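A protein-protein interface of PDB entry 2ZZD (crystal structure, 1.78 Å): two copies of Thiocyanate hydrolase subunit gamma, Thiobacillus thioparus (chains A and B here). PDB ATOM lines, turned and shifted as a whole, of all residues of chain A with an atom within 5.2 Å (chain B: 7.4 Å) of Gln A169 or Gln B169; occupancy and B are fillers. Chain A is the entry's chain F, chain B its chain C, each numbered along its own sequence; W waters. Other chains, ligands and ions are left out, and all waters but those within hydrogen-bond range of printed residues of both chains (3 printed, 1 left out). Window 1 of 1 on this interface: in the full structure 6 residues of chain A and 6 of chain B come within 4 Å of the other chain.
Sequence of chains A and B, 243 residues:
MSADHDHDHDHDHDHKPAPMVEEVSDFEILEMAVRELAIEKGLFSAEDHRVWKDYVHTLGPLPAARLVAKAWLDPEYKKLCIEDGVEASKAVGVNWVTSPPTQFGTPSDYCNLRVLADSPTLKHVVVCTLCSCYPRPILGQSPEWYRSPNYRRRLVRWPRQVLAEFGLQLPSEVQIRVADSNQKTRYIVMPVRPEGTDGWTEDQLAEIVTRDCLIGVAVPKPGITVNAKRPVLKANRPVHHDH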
ATOM      1  N   ARG A 160      17.215  20.044  18.737  1.00  0.00           N
ATOM      2  CA  ARG A 160      17.817  21.193  18.078  1.00  0.00           C
ATOM      3  C   ARG A 160      19.262  20.944  17.684  1.00  0.00           C
ATOM      4  O   ARG A 160      19.726  21.456  16.666  1.00  0.00           O
ATOM      5  CB  ARG A 160      17.699  22.430  18.955  1.00  0.00           C
ATOM      6  CG  ARG A 160      16.277  22.962  18.965  1.00  0.00           C
ATOM      7  CD  ARG A 160      16.162  24.227  19.765  1.00  0.00           C
ATOM      8  NE  ARG A 160      14.771  24.628  19.929  1.00  0.00           N
ATOM      9  CZ  ARG A 160      14.170  25.572  19.212  1.00  0.00           C
ATOM     10  NH1 ARG A 160      14.834  26.226  18.266  1.00  0.00           N
ATOM     11  NH2 ARG A 160      12.903  25.871  19.456  1.00  0.00           N
ATOM     12  N   LEU A 163      19.024  18.482  14.636  1.00  0.00           N
ATOM     13  CA  LEU A 163      18.561  19.204  13.456  1.00  0.00           C
ATOM     14  C   LEU A 163      19.660  20.124  12.923  1.00  0.00           C
ATOM     15  O   LEU A 163      19.833  20.261  11.714  1.00  0.00           O
ATOM     16  CB  LEU A 163      17.299  20.013  13.777  1.00  0.00           C
ATOM     17  CG  LEU A 163      16.018  19.195  13.981  1.00  0.00           C
ATOM     18  CD1 LEU A 163      14.857  20.125  14.320  1.00  0.00           C
ATOM     19  CD2 LEU A 163      15.712  18.397  12.718  1.00  0.00           C
ATOM     20  N   GLY A 167      21.581  20.638   9.330  1.00  0.00           N
ATOM     21  CA  GLY A 167      21.576  21.933   8.674  1.00  0.00           C
ATOM     22  C   GLY A 167      20.292  22.729   8.838  1.00  0.00           C
ATOM     23  O   GLY A 167      20.036  23.654   8.067  1.00  0.00           O
ATOM     24  N   LEU A 168      19.487  22.385   9.840  1.00  0.00           N
ATOM     25  CA  LEU A 168      18.228  23.082  10.088  1.00  0.00           C
ATOM     26  C   LEU A 168      18.193  23.718  11.470  1.00  0.00           C
ATOM     27  O   LEU A 168      18.476  23.065  12.474  1.00  0.00           O
ATOM     28  CB  LEU A 168      17.051  22.113   9.937  1.00  0.00           C
ATOM     29  CG  LEU A 168      15.658  22.657  10.276  1.00  0.00           C
ATOM     30  CD1 LEU A 168      15.306  23.815   9.351  1.00  0.00           C
ATOM     31  CD2 LEU A 168      14.632  21.541  10.139  1.00  0.00           C
ATOM     32  N   GLN A 169      17.832  24.997  11.504  1.00  0.00           N
ATOM     33  CA  GLN A 169      17.757  25.735  12.750  1.00  0.00           C
ATOM     34  C   GLN A 169      16.500  26.582  12.764  1.00  0.00           C
ATOM     35  O   GLN A 169      16.122  27.192  11.762  1.00  0.00           O
ATOM     36  CB  GLN A 169      18.990  26.631  12.902  1.00  0.00           C
ATOM     37  CG  GLN A 169      19.106  27.357  14.235  1.00  0.00           C
ATOM     38  CD  GLN A 169      20.466  28.030  14.408  1.00  0.00           C
ATOM     39  OE1 GLN A 169      21.363  27.501  15.074  1.00  0.00           O
ATOM     40  NE2 GLN A 169      20.627  29.194  13.790  1.00  0.00           N
ATOM     41  N   LEU A 170      15.848  26.622  13.911  1.00  0.00           N
ATOM     42  CA  LEU A 170      14.638  27.400  14.027  1.00  0.00           C
ATOM     43  C   LEU A 170      14.737  28.405  15.155  1.00  0.00           C
ATOM     44  O   LEU A 170      15.528  28.216  16.072  1.00  0.00           O
ATOM     45  CB  LEU A 170      13.459  26.449  14.219  1.00  0.00           C
ATOM     46  CG  LEU A 170      13.170  25.911  12.842  1.00  0.00           C
ATOM     47  CD1 LEU A 170      13.224  24.402  12.796  1.00  0.00           C
ATOM     48  CD2 LEU A 170      11.852  26.470  12.361  1.00  0.00           C
ATOM     49  N   PRO A 171      13.925  29.478  15.109  1.00  0.00           N
ATOM     50  CA  PRO A 171      13.997  30.467  16.188  1.00  0.00           C
ATOM     51  C   PRO A 171      13.832  29.773  17.544  1.00  0.00           C
ATOM     52  O   PRO A 171      13.094  28.786  17.668  1.00  0.00           O
ATOM     53  CB  PRO A 171      12.836  31.399  15.873  1.00  0.00           C
ATOM     54  CG  PRO A 171      12.784  31.351  14.371  1.00  0.00           C
ATOM     55  CD  PRO A 171      12.910  29.864  14.113  1.00  0.00           C
ATOM     56  N   SER A 172      14.494  30.299  18.568  1.00  0.00           N
ATOM     57  CA  SER A 172      14.419  29.693  19.892  1.00  0.00           C
ATOM     58  C   SER A 172      13.016  29.685  20.477  1.00  0.00           C
ATOM     59  O   SER A 172      12.676  28.796  21.251  1.00  0.00           O
ATOM     60  CB  SER A 172      15.375  30.401  20.857  1.00  0.00           C
ATOM     61  OG  SER A 172      15.052  31.774  20.990  1.00  0.00           O
ATOM     62  N   ARG B 160      27.933  24.916  17.380  1.00  0.00           N
ATOM     63  CA  ARG B 160      26.523  25.296  17.342  1.00  0.00           C
ATOM     64  C   ARG B 160      25.719  24.411  18.291  1.00  0.00           C
ATOM     65  O   ARG B 160      24.823  24.881  18.995  1.00  0.00           O
ATOM     66  CB  ARG B 160      25.976  25.137  15.924  1.00  0.00           C
ATOM     67  CG  ARG B 160      26.650  26.036  14.893  1.00  0.00           C
ATOM     68  CD  ARG B 160      25.859  27.308  14.697  1.00  0.00           C
ATOM     69  NE  ARG B 160      26.487  28.236  13.762  1.00  0.00           N
ATOM     70  CZ  ARG B 160      25.981  29.429  13.464  1.00  0.00           C
ATOM     71  NH1 ARG B 160      24.847  29.822  14.028  1.00  0.00           N
ATOM     72  NH2 ARG B 160      26.608  30.229  12.612  1.00  0.00           N
ATOM     73  N   GLN B 161      26.052  23.125  18.304  1.00  0.00           N
ATOM     74  CA  GLN B 161      25.360  22.174  19.157  1.00  0.00           C
ATOM     75  C   GLN B 161      25.715  22.381  20.630  1.00  0.00           C
ATOM     76  O   GLN B 161      24.834  22.392  21.491  1.00  0.00           O
ATOM     77  CB  GLN B 161      25.683  20.742  18.720  1.00  0.00           C
ATOM     78  CG  GLN B 161      25.145  20.356  17.334  1.00  0.00           C
ATOM     79  CD  GLN B 161      25.962  20.927  16.186  1.00  0.00           C
ATOM     80  OE1 GLN B 161      27.059  21.446  16.386  1.00  0.00           O
ATOM     81  NE2 GLN B 161      25.432  20.823  14.971  1.00  0.00           N
ATOM     82  N   LEU B 163      26.872  25.138  22.028  1.00  0.00           N
ATOM     83  CA  LEU B 163      26.315  26.410  22.464  1.00  0.00           C
ATOM     84  C   LEU B 163      24.809  26.298  22.695  1.00  0.00           C
ATOM     85  O   LEU B 163      24.275  26.896  23.627  1.00  0.00           O
ATOM     86  CB  LEU B 163      26.620  27.513  21.447  1.00  0.00           C
ATOM     87  CG  LEU B 163      28.085  27.975  21.420  1.00  0.00           C
ATOM     88  CD1 LEU B 163      28.287  29.021  20.326  1.00  0.00           C
ATOM     89  CD2 LEU B 163      28.466  28.555  22.780  1.00  0.00           C
ATOM     90  N   ALA B 164      24.122  25.529  21.852  1.00  0.00           N
ATOM     91  CA  ALA B 164      22.681  25.352  22.014  1.00  0.00           C
ATOM     92  C   ALA B 164      22.391  24.685  23.357  1.00  0.00           C
ATOM     93  O   ALA B 164      21.403  25.003  24.020  1.00  0.00           O
ATOM     94  CB  ALA B 164      22.113  24.512  20.872  1.00  0.00           C
ATOM     95  N   PHE B 166      24.018  25.104  25.965  1.00  0.00           N
ATOM     96  CA  PHE B 166      24.197  26.166  26.951  1.00  0.00           C
ATOM     97  C   PHE B 166      23.060  27.182  26.881  1.00  0.00           C
ATOM     98  O   PHE B 166      22.989  28.098  27.704  1.00  0.00           O
ATOM     99  CB  PHE B 166      25.521  26.906  26.731  1.00  0.00           C
ATOM    100  CG  PHE B 166      26.703  26.259  27.394  1.00  0.00           C
ATOM    101  CD1 PHE B 166      27.554  25.425  26.674  1.00  0.00           C
ATOM    102  CD2 PHE B 166      26.980  26.502  28.736  1.00  0.00           C
ATOM    103  CE1 PHE B 166      28.668  24.841  27.282  1.00  0.00           C
ATOM    104  CE2 PHE B 166      28.091  25.924  29.353  1.00  0.00           C
ATOM    105  CZ  PHE B 166      28.934  25.094  28.627  1.00  0.00           C
ATOM    106  N   GLY B 167      22.187  27.024  25.889  1.00  0.00           N
ATOM    107  CA  GLY B 167      21.064  27.934  25.731  1.00  0.00           C
ATOM    108  C   GLY B 167      21.341  29.115  24.816  1.00  0.00           C
ATOM    109  O   GLY B 167      20.623  30.115  24.858  1.00  0.00           O
ATOM    110  N   LEU B 168      22.375  29.002  23.987  1.00  0.00           N
ATOM    111  CA  LEU B 168      22.747  30.076  23.070  1.00  0.00           C
ATOM    112  C   LEU B 168      22.677  29.672  21.603  1.00  0.00           C
ATOM    113  O   LEU B 168      23.270  28.680  21.184  1.00  0.00           O
ATOM    114  CB  LEU B 168      24.160  30.568  23.388  1.00  0.00           C
ATOM    115  CG  LEU B 168      24.745  31.636  22.462  1.00  0.00           C
ATOM    116  CD1 LEU B 168      23.886  32.891  22.509  1.00  0.00           C
ATOM    117  CD2 LEU B 168      26.172  31.951  22.892  1.00  0.00           C
ATOM    118  N   GLN B 169      21.957  30.466  20.820  1.00  0.00           N
ATOM    119  CA  GLN B 169      21.808  30.193  19.405  1.00  0.00           C
ATOM    120  C   GLN B 169      22.022  31.471  18.614  1.00  0.00           C
ATOM    121  O   GLN B 169      21.588  32.544  19.019  1.00  0.00           O
ATOM    122  CB  GLN B 169      20.407  29.651  19.126  1.00  0.00           C
ATOM    123  CG  GLN B 169      20.226  29.020  17.762  1.00  0.00           C
ATOM    124  CD  GLN B 169      18.873  28.330  17.632  1.00  0.00           C
ATOM    125  OE1 GLN B 169      17.827  28.981  17.627  1.00  0.00           O
ATOM    126  NE2 GLN B 169      18.891  27.003  17.544  1.00  0.00           N
ATOM    127  N   LEU B 170      22.693  31.357  17.483  1.00  0.00           N
ATOM    128  CA  LEU B 170      22.928  32.530  16.670  1.00  0.00           C
ATOM    129  C   LEU B 170      22.441  32.312  15.257  1.00  0.00           C
ATOM    130  O   LEU B 170      22.324  31.174  14.815  1.00  0.00           O
ATOM    131  CB  LEU B 170      24.417  32.884  16.701  1.00  0.00           C
ATOM    132  CG  LEU B 170      24.603  33.551  18.048  1.00  0.00           C
ATOM    133  CD1 LEU B 170      25.573  32.790  18.923  1.00  0.00           C
ATOM    134  CD2 LEU B 170      25.010  34.993  17.847  1.00  0.00           C
ATOM    135  N   PRO B 171      22.149  33.406  14.526  1.00  0.00           N
ATOM    136  CA  PRO B 171      21.678  33.234  13.149  1.00  0.00           C
ATOM    137  C   PRO B 171      22.668  32.347  12.388  1.00  0.00           C
ATOM    138  O   PRO B 171      23.880  32.398  12.633  1.00  0.00           O
ATOM    139  CB  PRO B 171      21.658  34.659  12.614  1.00  0.00           C
ATOM    140  CG  PRO B 171      21.318  35.461  13.834  1.00  0.00           C
ATOM    141  CD  PRO B 171      22.234  34.837  14.873  1.00  0.00           C
ATOM    142  N   SER B 172      22.166  31.552  11.452  1.00  0.00           N
ATOM    143  CA  SER B 172      23.032  30.658  10.701  1.00  0.00           C
ATOM    144  C   SER B 172      24.079  31.382   9.865  1.00  0.00           C
ATOM    145  O   SER B 172      25.145  30.830   9.597  1.00  0.00           O
ATOM    146  CB  SER B 172      22.197  29.739   9.803  1.00  0.00           C
ATOM    147  OG  SER B 172      21.452  30.484   8.860  1.00  0.00           O
ATOM    148  N   GLU B 173      23.782  32.618   9.466  1.00  0.00           N
ATOM    149  CA  GLU B 173      24.709  33.390   8.644  1.00  0.00           C
ATOM    150  C   GLU B 173      25.826  34.046   9.452  1.00  0.00           C
ATOM    151  O   GLU B 173      26.857  34.437   8.897  1.00  0.00           O
ATOM    152  CB  GLU B 173      23.955  34.464   7.851  1.00  0.00           C
ATOM    153  CG  GLU B 173      23.316  35.543   8.710  1.00  0.00           C
ATOM    154  CD  GLU B 173      21.875  35.239   9.076  1.00  0.00           C
ATOM    155  OE1 GLU B 173      21.481  34.053   9.026  1.00  0.00           O
ATOM    156  OE2 GLU B 173      21.142  36.191   9.422  1.00  0.00           O
ATOM    157  N   ILE B 176      30.368  31.980  13.703  1.00  0.00           N
ATOM    158  CA  ILE B 176      30.714  31.618  15.063  1.00  0.00           C
ATOM    159  C   ILE B 176      32.173  31.215  14.932  1.00  0.00           C
ATOM    160  O   ILE B 176      32.516  30.380  14.091  1.00  0.00           O
ATOM    161  CB  ILE B 176      29.875  30.435  15.603  1.00  0.00           C
ATOM    162  CG1 ILE B 176      28.454  30.909  15.934  1.00  0.00           C
ATOM    163  CG2 ILE B 176      30.527  29.866  16.867  1.00  0.00           C
ATOM    164  CD1 ILE B 176      27.564  29.831  16.544  1.00  0.00           C
ATOM    165  N   VAL B 217      29.989  31.279  26.127  1.00  0.00           N
ATOM    166  CA  VAL B 217      28.892  30.313  26.117  1.00  0.00           C
ATOM    167  C   VAL B 217      27.546  30.962  26.442  1.00  0.00           C
ATOM    168  O   VAL B 217      26.512  30.291  26.472  1.00  0.00           O
ATOM    169  CB  VAL B 217      29.153  29.144  27.098  1.00  0.00           C
ATOM    170  CG1 VAL B 217      30.413  28.400  26.685  1.00  0.00           C
ATOM    171  CG2 VAL B 217      29.294  29.664  28.521  1.00  0.00           C
ATOM    172  N   VAL B 219      25.460  35.184  26.299  1.00  0.00           N
ATOM    173  CA  VAL B 219      25.542  36.578  25.877  1.00  0.00           C
ATOM    174  C   VAL B 219      24.875  37.397  26.971  1.00  0.00           C
ATOM    175  O   VAL B 219      23.977  36.913  27.661  1.00  0.00           O
ATOM    176  CB  VAL B 219      24.829  36.861  24.522  1.00  0.00           C
ATOM    177  CG1 VAL B 219      25.653  36.306  23.378  1.00  0.00           C
ATOM    178  CG2 VAL B 219      23.435  36.259  24.522  1.00  0.00           C
HETATM  179  O   HOH W   1      20.975  25.335  16.859  1.00  0.00           O
HETATM  180  O   HOH W   2      22.274  23.132  17.871  1.00  0.00           O
HETATM  181  O   HOH W   3      23.477  28.722  16.512  1.00  0.00           O
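Among the printed residues, pairs that only touch across the chains: Gln A169 with Gln B169 (3.3 Å), Gln A169 with Ser B172 (3.7 Å) and Ser A172 with Gln B169 (3.7 Å).
The guanidinium group (NH2) of Arg B160 is in hydrogen-bond range of the backbone carbonyl oxygen (O) of Ser B172 (3.4 Å). The guanidinium group of Arg B160 lies within hydrogen-bond range of the backbone carbonyl oxygen of Leu B170 (3.0 Å). NH2 of Arg A160 lies within hydrogen-bond range of O of Ser A172 (3.4 Å). The guanidinium group (NH1) of Arg A160 lies within hydrogen-bond range of the backbone carbonyl oxygen (O) of Leu A170.
Along chain B the printed residues that touch a printed residue of chain A span positions 169 to 172. Among the printed residues, no Asp or Glu carboxylate lies within 4 Å of a Lys or Arg side-chain nitrogen of the other chain.
Printed residues of chain B within 4 Å of Leu A170: Gln B169. Of the printed residues of chain B, Ser A172 touches Gln B169. Of the printed residues of chain A, Gln B169 touches Gln A169 (3.3 Å), Leu A170 (2.9 Å) and Ser A172 (3.7 Å). Of the printed residues of chain A, Leu B170 touches Gln A169 (2.8 Å). Of the printed residues of chain A, Ser B172 touches Gln A169 (3.7 Å). The nearest printed residue of chain B that does not touch Gln A169 is Pro B171 (4.01 Å). The nearest residue of chain A that does not touch Gln B169 is Pro A171 (4.1 Å).
Water W1 bridges NE2 of Gln B169 (2.8 Å) and OE1 of Gln A169 (2.8 Å). Water W3 lies within hydrogen-bond range of OE1 of Gln A169 (2.8 Å), N of Leu B170 (2.9 Å) and NH1 of Arg B160 (3.0 Å). Water W2 lies within hydrogen-bond range of O of Arg A160 (3.3 Å) and O of Arg B160 (3.3 Å).
Gln B169 touches its own counterpart, Gln A169. Gln A169 touches Leu B170, and with the chains exchanged Leu A170 touches Gln B169. Gln A169 touches Ser B172, and with the chains exchanged Ser A172 touches Gln B169. Positions printed for both chains: 160, 163, 167, 168, 169, 170, 171 and 172. Of the 5 pairs that touch across the chains among the printed residues, 5 have their exchanged pair printed and touching as well.
O of Leu B170 sits at hydrogen-bond distance from NE2 of Gln A169, at 2.8 Å. O of Leu A170 sits close to OE1 of Gln B169, at 2.9 Å.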
